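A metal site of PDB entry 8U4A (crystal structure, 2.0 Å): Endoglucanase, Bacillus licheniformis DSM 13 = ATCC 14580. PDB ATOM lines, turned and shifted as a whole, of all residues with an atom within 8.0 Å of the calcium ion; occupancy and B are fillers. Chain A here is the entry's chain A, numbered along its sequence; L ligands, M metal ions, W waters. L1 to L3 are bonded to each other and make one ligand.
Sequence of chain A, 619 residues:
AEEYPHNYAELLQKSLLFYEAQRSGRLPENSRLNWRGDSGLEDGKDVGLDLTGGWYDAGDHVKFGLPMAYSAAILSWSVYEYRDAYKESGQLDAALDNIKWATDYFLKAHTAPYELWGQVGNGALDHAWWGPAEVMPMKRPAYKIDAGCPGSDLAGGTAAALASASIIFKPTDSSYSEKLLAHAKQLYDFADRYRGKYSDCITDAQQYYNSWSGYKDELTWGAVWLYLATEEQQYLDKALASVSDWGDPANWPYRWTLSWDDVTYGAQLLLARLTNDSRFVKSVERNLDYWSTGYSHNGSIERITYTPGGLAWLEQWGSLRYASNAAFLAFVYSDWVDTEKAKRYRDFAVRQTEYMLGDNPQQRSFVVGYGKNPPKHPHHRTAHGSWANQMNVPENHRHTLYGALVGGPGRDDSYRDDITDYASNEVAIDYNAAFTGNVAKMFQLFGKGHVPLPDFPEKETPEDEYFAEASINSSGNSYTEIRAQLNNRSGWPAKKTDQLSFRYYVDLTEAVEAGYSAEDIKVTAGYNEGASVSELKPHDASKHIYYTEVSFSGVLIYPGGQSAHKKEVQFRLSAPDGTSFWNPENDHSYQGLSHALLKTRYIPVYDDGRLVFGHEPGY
An oxygen (O6) of LIG L1 sits at hydrogen-bond distance from the side-chain hydroxyl (OG) of Ser 259 (3.3 Å). An oxygen (O1) of LG2 L2 is in hydrogen-bond range of the side-chain carboxylate (OD2) of Asp 261 (2.7 Å). OD2 of Asp 262 sits at hydrogen-bond distance from O2 of LG2 L2 (2.6 Å).
The backbone NH (N) of Val 263 lies close to the side-chain carboxylate (OD2) of Asp 217, 2.9 Å away. The side-chain hydroxyl (OG) of Ser 211 is in hydrogen-bond range of the backbone NH (N) of Gly 214, 3.3 Å away. N of Trp 212 lies within hydrogen-bond range of OD1 of Asp 261 (3.1 Å).
The nearest printed residue that does not touch the calcium ion is Asp 262 (4.3 Å).
The calcium ion is bound by the side-chain carboxylate (OE1) of Glu 218 (2.4 Å), the backbone carbonyl oxygen (O) of Gly 214 (2.4 Å), the side-chain hydroxyl (OG) of Ser 213 (2.4 Å), water W1 (2.4 Å), the backbone carbonyl oxygen (O) of Asp 261 (2.5 Å), the side-chain carboxylate (OD1) of Asp 217 (2.5 Å), the side-chain carboxylate (OE2) of Glu 218 (2.5 Å) and the side-chain carboxylate (OD2) of Asp 217 (2.5 Å).
Water W1 bridges the side-chain carboxylate of Asp 261 (2.6 Å) and the side-chain hydroxyl of Ser 211 (2.8 Å).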
ATOM      1  N   LEU A  66     -36.174  19.578 -12.477  1.00  0.00           N
ATOM      2  CA  LEU A  66     -35.422  20.050 -11.300  1.00  0.00           C
ATOM      3  C   LEU A  66     -36.341  20.866 -10.407  1.00  0.00           C
ATOM      4  O   LEU A  66     -36.458  20.532  -9.216  1.00  0.00           O
ATOM      5  CB  LEU A  66     -34.155  20.826 -11.714  1.00  0.00           C
ATOM      6  CG  LEU A  66     -33.293  21.289 -10.509  1.00  0.00           C
ATOM      7  CD1 LEU A  66     -32.643  20.060  -9.932  1.00  0.00           C
ATOM      8  CD2 LEU A  66     -32.211  22.291 -10.912  1.00  0.00           C
ATOM      9  N   SER A 152     -26.328  15.130 -11.312  1.00  0.00           N
ATOM     10  CA  SER A 152     -26.277  14.952  -9.874  1.00  0.00           C
ATOM     11  C   SER A 152     -27.225  15.881  -9.166  1.00  0.00           C
ATOM     12  O   SER A 152     -27.747  15.549  -8.096  1.00  0.00           O
ATOM     13  CB  SER A 152     -24.844  15.187  -9.371  1.00  0.00           C
ATOM     14  OG  SER A 152     -23.972  14.216  -9.906  1.00  0.00           O
ATOM     15  N   ASP A 153     -27.469  17.054  -9.756  1.00  0.00           N
ATOM     16  CA  ASP A 153     -28.440  17.978  -9.169  1.00  0.00           C
ATOM     17  C   ASP A 153     -29.857  17.458  -9.344  1.00  0.00           C
ATOM     18  O   ASP A 153     -30.616  17.341  -8.375  1.00  0.00           O
ATOM     19  CB  ASP A 153     -28.268  19.405  -9.758  1.00  0.00           C
ATOM     20  CG  ASP A 153     -27.793  19.405 -11.224  1.00  0.00           C
ATOM     21  OD1 ASP A 153     -28.033  18.435 -11.974  1.00  0.00           O
ATOM     22  OD2 ASP A 153     -27.143  20.410 -11.639  1.00  0.00           O
ATOM     23  N   LEU A 154     -30.245  17.142 -10.580  1.00  0.00           N
ATOM     24  CA  LEU A 154     -31.572  16.591 -10.824  1.00  0.00           C
ATOM     25  C   LEU A 154     -31.791  15.277 -10.055  1.00  0.00           C
ATOM     26  O   LEU A 154     -32.843  15.060  -9.423  1.00  0.00           O
ATOM     27  CB  LEU A 154     -31.763  16.393 -12.328  1.00  0.00           C
ATOM     28  CG  LEU A 154     -33.068  15.658 -12.712  1.00  0.00           C
ATOM     29  CD1 LEU A 154     -34.275  16.565 -12.345  1.00  0.00           C
ATOM     30  CD2 LEU A 154     -33.051  15.259 -14.204  1.00  0.00           C
ATOM     31  N   LYS A 197     -23.669  18.284 -14.023  1.00  0.00           N
ATOM     32  CA  LYS A 197     -24.861  19.148 -13.991  1.00  0.00           C
ATOM     33  C   LYS A 197     -25.878  18.663 -15.016  1.00  0.00           C
ATOM     34  O   LYS A 197     -25.536  18.461 -16.187  1.00  0.00           O
ATOM     35  CB  LYS A 197     -24.479  20.597 -14.284  1.00  0.00           C
ATOM     36  CG  LYS A 197     -23.491  21.192 -13.291  1.00  0.00           C
ATOM     37  CD  LYS A 197     -23.384  22.688 -13.466  1.00  0.00           C
ATOM     38  CE  LYS A 197     -22.426  23.096 -14.531  1.00  0.00           C
ATOM     39  NZ  LYS A 197     -22.102  24.567 -14.453  1.00  0.00           N
ATOM     40  N   ASN A 210     -31.472  26.539 -15.637  1.00  0.00           N
ATOM     41  CA  ASN A 210     -30.053  26.244 -15.699  1.00  0.00           C
ATOM     42  C   ASN A 210     -29.561  25.915 -14.283  1.00  0.00           C
ATOM     43  O   ASN A 210     -30.044  26.465 -13.275  1.00  0.00           O
ATOM     44  CB  ASN A 210     -29.324  27.446 -16.292  1.00  0.00           C
ATOM     45  CG  ASN A 210     -27.847  27.175 -16.458  1.00  0.00           C
ATOM     46  OD1 ASN A 210     -27.494  26.148 -16.980  1.00  0.00           O
ATOM     47  ND2 ASN A 210     -26.981  28.106 -15.994  1.00  0.00           N
ATOM     48  N   SER A 211     -28.583  25.010 -14.216  1.00  0.00           N
ATOM     49  CA  SER A 211     -27.976  24.654 -12.925  1.00  0.00           C
ATOM     50  C   SER A 211     -26.946  25.737 -12.579  1.00  0.00           C
ATOM     51  O   SER A 211     -25.743  25.587 -12.768  1.00  0.00           O
ATOM     52  CB  SER A 211     -27.342  23.275 -12.944  1.00  0.00           C
ATOM     53  OG  SER A 211     -26.810  22.958 -11.631  1.00  0.00           O
ATOM     54  N   TRP A 212     -27.453  26.870 -12.091  1.00  0.00           N
ATOM     55  CA  TRP A 212     -26.556  27.986 -11.772  1.00  0.00           C
ATOM     56  C   TRP A 212     -25.539  27.581 -10.723  1.00  0.00           C
ATOM     57  O   TRP A 212     -24.343  27.778 -10.904  1.00  0.00           O
ATOM     58  CB  TRP A 212     -27.351  29.190 -11.304  1.00  0.00           C
ATOM     59  CG  TRP A 212     -28.351  29.665 -12.343  1.00  0.00           C
ATOM     60  CD1 TRP A 212     -29.688  29.378 -12.384  1.00  0.00           C
ATOM     61  CD2 TRP A 212     -28.063  30.447 -13.516  1.00  0.00           C
ATOM     62  NE1 TRP A 212     -30.252  29.963 -13.516  1.00  0.00           N
ATOM     63  CE2 TRP A 212     -29.283  30.643 -14.203  1.00  0.00           C
ATOM     64  CE3 TRP A 212     -26.892  31.024 -14.037  1.00  0.00           C
ATOM     65  CZ2 TRP A 212     -29.376  31.368 -15.378  1.00  0.00           C
ATOM     66  CZ3 TRP A 212     -26.981  31.749 -15.220  1.00  0.00           C
ATOM     67  CH2 TRP A 212     -28.212  31.922 -15.870  1.00  0.00           C
ATOM     68  N   SER A 213     -25.987  26.936  -9.629  1.00  0.00           N
ATOM     69  CA  SER A 213     -25.171  26.659  -8.470  1.00  0.00           C
ATOM     70  C   SER A 213     -24.388  25.347  -8.595  1.00  0.00           C
ATOM     71  O   SER A 213     -23.502  25.086  -7.755  1.00  0.00           O
ATOM     72  CB  SER A 213     -26.045  26.581  -7.223  1.00  0.00           C
ATOM     73  OG  SER A 213     -27.009  25.536  -7.361  1.00  0.00           O
ATOM     74  N   GLY A 214     -24.683  24.518  -9.585  1.00  0.00           N
ATOM     75  CA  GLY A 214     -24.008  23.235  -9.604  1.00  0.00           C
ATOM     76  C   GLY A 214     -24.751  22.256  -8.724  1.00  0.00           C
ATOM     77  O   GLY A 214     -25.881  22.499  -8.300  1.00  0.00           O
ATOM     78  N   TYR A 215     -24.122  21.112  -8.441  1.00  0.00           N
ATOM     79  CA  TYR A 215     -24.833  19.998  -7.815  1.00  0.00           C
ATOM     80  C   TYR A 215     -24.343  19.692  -6.410  1.00  0.00           C
ATOM     81  O   TYR A 215     -24.882  18.779  -5.775  1.00  0.00           O
ATOM     82  CB  TYR A 215     -24.721  18.735  -8.698  1.00  0.00           C
ATOM     83  CG  TYR A 215     -23.290  18.360  -9.077  1.00  0.00           C
ATOM     84  CD1 TYR A 215     -22.427  17.789  -8.137  1.00  0.00           C
ATOM     85  CD2 TYR A 215     -22.801  18.589 -10.353  1.00  0.00           C
ATOM     86  CE1 TYR A 215     -21.091  17.461  -8.469  1.00  0.00           C
ATOM     87  CE2 TYR A 215     -21.458  18.267 -10.682  1.00  0.00           C
ATOM     88  CZ  TYR A 215     -20.624  17.698  -9.744  1.00  0.00           C
ATOM     89  OH  TYR A 215     -19.318  17.335 -10.070  1.00  0.00           O
ATOM     90  N   LYS A 216     -23.335  20.405  -5.911  1.00  0.00           N
ATOM     91  CA  LYS A 216     -22.830  20.088  -4.576  1.00  0.00           C
ATOM     92  C   LYS A 216     -23.916  20.215  -3.519  1.00  0.00           C
ATOM     93  O   LYS A 216     -23.919  19.475  -2.533  1.00  0.00           O
ATOM     94  CB  LYS A 216     -21.642  20.988  -4.208  1.00  0.00           C
ATOM     95  CG  LYS A 216     -20.377  20.693  -4.957  1.00  0.00           C
ATOM     96  CD  LYS A 216     -19.356  21.873  -4.778  1.00  0.00           C
ATOM     97  CE  LYS A 216     -17.992  21.603  -5.481  1.00  0.00           C
ATOM     98  NZ  LYS A 216     -17.073  22.776  -5.403  1.00  0.00           N
ATOM     99  N   ASP A 217     -24.832  21.159  -3.699  1.00  0.00           N
ATOM    100  CA  ASP A 217     -25.864  21.342  -2.681  1.00  0.00           C
ATOM    101  C   ASP A 217     -26.875  20.187  -2.723  1.00  0.00           C
ATOM    102  O   ASP A 217     -27.330  19.722  -1.660  1.00  0.00           O
ATOM    103  CB  ASP A 217     -26.559  22.703  -2.856  1.00  0.00           C
ATOM    104  CG  ASP A 217     -26.983  22.993  -4.308  1.00  0.00           C
ATOM    105  OD1 ASP A 217     -26.118  22.992  -5.209  1.00  0.00           O
ATOM    106  OD2 ASP A 217     -28.190  23.265  -4.546  1.00  0.00           O
ATOM    107  N   GLU A 218     -27.264  19.726  -3.921  1.00  0.00           N
ATOM    108  CA  GLU A 218     -28.212  18.606  -4.010  1.00  0.00           C
ATOM    109  C   GLU A 218     -27.588  17.312  -3.491  1.00  0.00           C
ATOM    110  O   GLU A 218     -28.296  16.445  -2.955  1.00  0.00           O
ATOM    111  CB  GLU A 218     -28.678  18.417  -5.475  1.00  0.00           C
ATOM    112  CG  GLU A 218     -29.675  19.492  -5.942  1.00  0.00           C
ATOM    113  CD  GLU A 218     -29.041  20.797  -6.476  1.00  0.00           C
ATOM    114  OE1 GLU A 218     -27.793  20.889  -6.625  1.00  0.00           O
ATOM    115  OE2 GLU A 218     -29.807  21.732  -6.796  1.00  0.00           O
ATOM    116  N   LEU A 219     -26.282  17.151  -3.634  1.00  0.00           N
ATOM    117  CA  LEU A 219     -25.649  15.979  -3.041  1.00  0.00           C
ATOM    118  C   LEU A 219     -25.828  15.962  -1.526  1.00  0.00           C
ATOM    119  O   LEU A 219     -26.156  14.917  -0.953  1.00  0.00           O
ATOM    120  CB  LEU A 219     -24.163  15.935  -3.415  1.00  0.00           C
ATOM    121  CG  LEU A 219     -23.918  15.561  -4.890  1.00  0.00           C
ATOM    122  CD1 LEU A 219     -22.399  15.482  -5.207  1.00  0.00           C
ATOM    123  CD2 LEU A 219     -24.660  14.242  -5.199  1.00  0.00           C
ATOM    124  N   SER A 259     -34.092  27.712  -2.859  1.00  0.00           N
ATOM    125  CA  SER A 259     -34.681  27.934  -4.169  1.00  0.00           C
ATOM    126  C   SER A 259     -34.570  26.636  -4.956  1.00  0.00           C
ATOM    127  O   SER A 259     -33.858  25.713  -4.549  1.00  0.00           O
ATOM    128  CB  SER A 259     -33.980  29.078  -4.920  1.00  0.00           C
ATOM    129  OG  SER A 259     -32.612  28.770  -5.061  1.00  0.00           O
ATOM    130  N   TRP A 260     -35.279  26.584  -6.099  1.00  0.00           N
ATOM    131  CA  TRP A 260     -35.248  25.380  -6.930  1.00  0.00           C
ATOM    132  C   TRP A 260     -33.830  25.031  -7.357  1.00  0.00           C
ATOM    133  O   TRP A 260     -33.507  23.849  -7.557  1.00  0.00           O
ATOM    134  CB  TRP A 260     -36.137  25.520  -8.182  1.00  0.00           C
ATOM    135  CG  TRP A 260     -35.754  26.688  -9.068  1.00  0.00           C
ATOM    136  CD1 TRP A 260     -36.278  27.932  -9.046  1.00  0.00           C
ATOM    137  CD2 TRP A 260     -34.719  26.696 -10.067  1.00  0.00           C
ATOM    138  NE1 TRP A 260     -35.608  28.755  -9.954  1.00  0.00           N
ATOM    139  CE2 TRP A 260     -34.663  27.999 -10.602  1.00  0.00           C
ATOM    140  CE3 TRP A 260     -33.821  25.720 -10.557  1.00  0.00           C
ATOM    141  CZ2 TRP A 260     -33.810  28.335 -11.641  1.00  0.00           C
ATOM    142  CZ3 TRP A 260     -32.949  26.078 -11.531  1.00  0.00           C
ATOM    143  CH2 TRP A 260     -32.935  27.363 -12.064  1.00  0.00           C
ATOM    144  N   ASP A 261     -32.952  26.037  -7.502  1.00  0.00           N
ATOM    145  CA  ASP A 261     -31.603  25.787  -7.947  1.00  0.00           C
ATOM    146  C   ASP A 261     -30.627  25.599  -6.810  1.00  0.00           C
ATOM    147  O   ASP A 261     -29.619  24.908  -6.998  1.00  0.00           O
ATOM    148  CB  ASP A 261     -31.063  26.942  -8.805  1.00  0.00           C
ATOM    149  CG  ASP A 261     -29.657  26.629  -9.336  1.00  0.00           C
ATOM    150  OD1 ASP A 261     -29.595  25.752 -10.196  1.00  0.00           O
ATOM    151  OD2 ASP A 261     -28.616  27.153  -8.816  1.00  0.00           O
ATOM    152  N   ASP A 262     -30.859  26.220  -5.652  1.00  0.00           N
ATOM    153  CA  ASP A 262     -29.862  26.185  -4.577  1.00  0.00           C
ATOM    154  C   ASP A 262     -30.513  25.691  -3.297  1.00  0.00           C
ATOM    155  O   ASP A 262     -31.248  26.422  -2.619  1.00  0.00           O
ATOM    156  CB  ASP A 262     -29.216  27.539  -4.377  1.00  0.00           C
ATOM    157  CG  ASP A 262     -27.919  27.443  -3.562  1.00  0.00           C
ATOM    158  OD1 ASP A 262     -27.858  26.463  -2.786  1.00  0.00           O
ATOM    159  OD2 ASP A 262     -27.019  28.320  -3.713  1.00  0.00           O
ATOM    160  N   VAL A 263     -30.268  24.428  -2.951  1.00  0.00           N
ATOM    161  CA  VAL A 263     -30.828  23.888  -1.708  1.00  0.00           C
ATOM    162  C   VAL A 263     -29.798  23.924  -0.572  1.00  0.00           C
ATOM    163  O   VAL A 263     -30.006  23.273   0.456  1.00  0.00           O
ATOM    164  CB  VAL A 263     -31.411  22.473  -1.925  1.00  0.00           C
ATOM    165  CG1 VAL A 263     -32.723  22.560  -2.691  1.00  0.00           C
ATOM    166  CG2 VAL A 263     -30.398  21.511  -2.648  1.00  0.00           C
ATOM    167  N   THR A 264     -28.683  24.645  -0.750  1.00  0.00           N
ATOM    168  CA  THR A 264     -27.741  24.738   0.370  1.00  0.00           C
ATOM    169  C   THR A 264     -28.450  25.130   1.632  1.00  0.00           C
ATOM    170  O   THR A 264     -28.188  24.585   2.715  1.00  0.00           O
ATOM    171  CB  THR A 264     -26.670  25.802   0.107  1.00  0.00           C
ATOM    172  OG1 THR A 264     -26.001  25.473  -1.106  1.00  0.00           O
ATOM    173  CG2 THR A 264     -25.709  25.830   1.222  1.00  0.00           C
HETATM  174  C1  LIG L   1     -31.717  33.227 -11.260  1.00  0.00           C
HETATM  175  C2  LIG L   1     -30.454  32.601 -10.677  1.00  0.00           C
HETATM  176  C3  LIG L   1     -30.745  31.834  -9.406  1.00  0.00           C
HETATM  177  C4  LIG L   1     -31.893  30.843  -9.626  1.00  0.00           C
HETATM  178  C5  LIG L   1     -32.329  30.121  -8.354  1.00  0.00           C
HETATM  179  C6  LIG L   1     -32.823  32.163 -11.398  1.00  0.00           C
HETATM  180  O1  LIG L   1     -34.004  32.751 -11.811  1.00  0.00           O
HETATM  181  O2  LIG L   1     -31.441  33.769 -12.546  1.00  0.00           O
HETATM  182  O3  LIG L   1     -29.438  33.580 -10.463  1.00  0.00           O
HETATM  183  O4  LIG L   1     -29.578  31.084  -9.103  1.00  0.00           O
HETATM  184  O5  LIG L   1     -33.050  31.534 -10.136  1.00  0.00           O
HETATM  185  O6  LIG L   1     -32.840  31.038  -7.391  1.00  0.00           O
HETATM  186  C1  LG2 L   2     -28.053  30.413  -7.378  1.00  0.00           C
HETATM  187  C2  LG2 L   2     -27.330  30.861  -6.127  1.00  0.00           C
HETATM  188  C3  LG2 L   2     -26.619  32.203  -6.326  1.00  0.00           C
HETATM  189  C4  LG2 L   2     -27.622  33.214  -6.897  1.00  0.00           C
HETATM  190  C5  LG2 L   2     -27.048  34.574  -7.236  1.00  0.00           C
HETATM  191  C6  LG2 L   2     -28.956  31.534  -7.887  1.00  0.00           C
HETATM  192  O1  LG2 L   2     -28.788  29.233  -7.107  1.00  0.00           O
HETATM  193  O2  LG2 L   2     -26.406  29.835  -5.780  1.00  0.00           O
HETATM  194  O3  LG2 L   2     -26.211  32.672  -5.065  1.00  0.00           O
HETATM  195  O4  LG2 L   2     -28.172  32.688  -8.115  1.00  0.00           O
HETATM  196  O5  LG2 L   2     -25.999  34.500  -8.198  1.00  0.00           O
HETATM  197  C1  LG3 L   3     -24.850  34.167  -3.782  1.00  0.00           C
HETATM  198  C2  LG3 L   3     -23.491  34.857  -3.749  1.00  0.00           C
HETATM  199  C3  LG3 L   3     -22.359  33.834  -3.891  1.00  0.00           C
HETATM  200  C4  LG3 L   3     -22.631  32.873  -5.063  1.00  0.00           C
HETATM  201  C5  LG3 L   3     -21.726  31.666  -5.073  1.00  0.00           C
HETATM  202  C6  LG3 L   3     -24.938  33.319  -5.041  1.00  0.00           C
HETATM  203  O1  LG3 L   3     -25.913  35.133  -3.820  1.00  0.00           O
HETATM  204  O2  LG3 L   3     -23.344  35.634  -2.565  1.00  0.00           O
HETATM  205  O3  LG3 L   3     -21.140  34.506  -4.188  1.00  0.00           O
HETATM  206  O4  LG3 L   3     -23.952  32.345  -5.006  1.00  0.00           O
HETATM  207  O5  LG3 L   3     -21.678  31.161  -6.400  1.00  0.00           O
HETATM  208 CA    CA M   1     -27.806  23.255  -7.045  1.00  0.00          CA
HETATM  209  O   HOH W   1     -28.406  23.540  -9.394  1.00  0.00           O
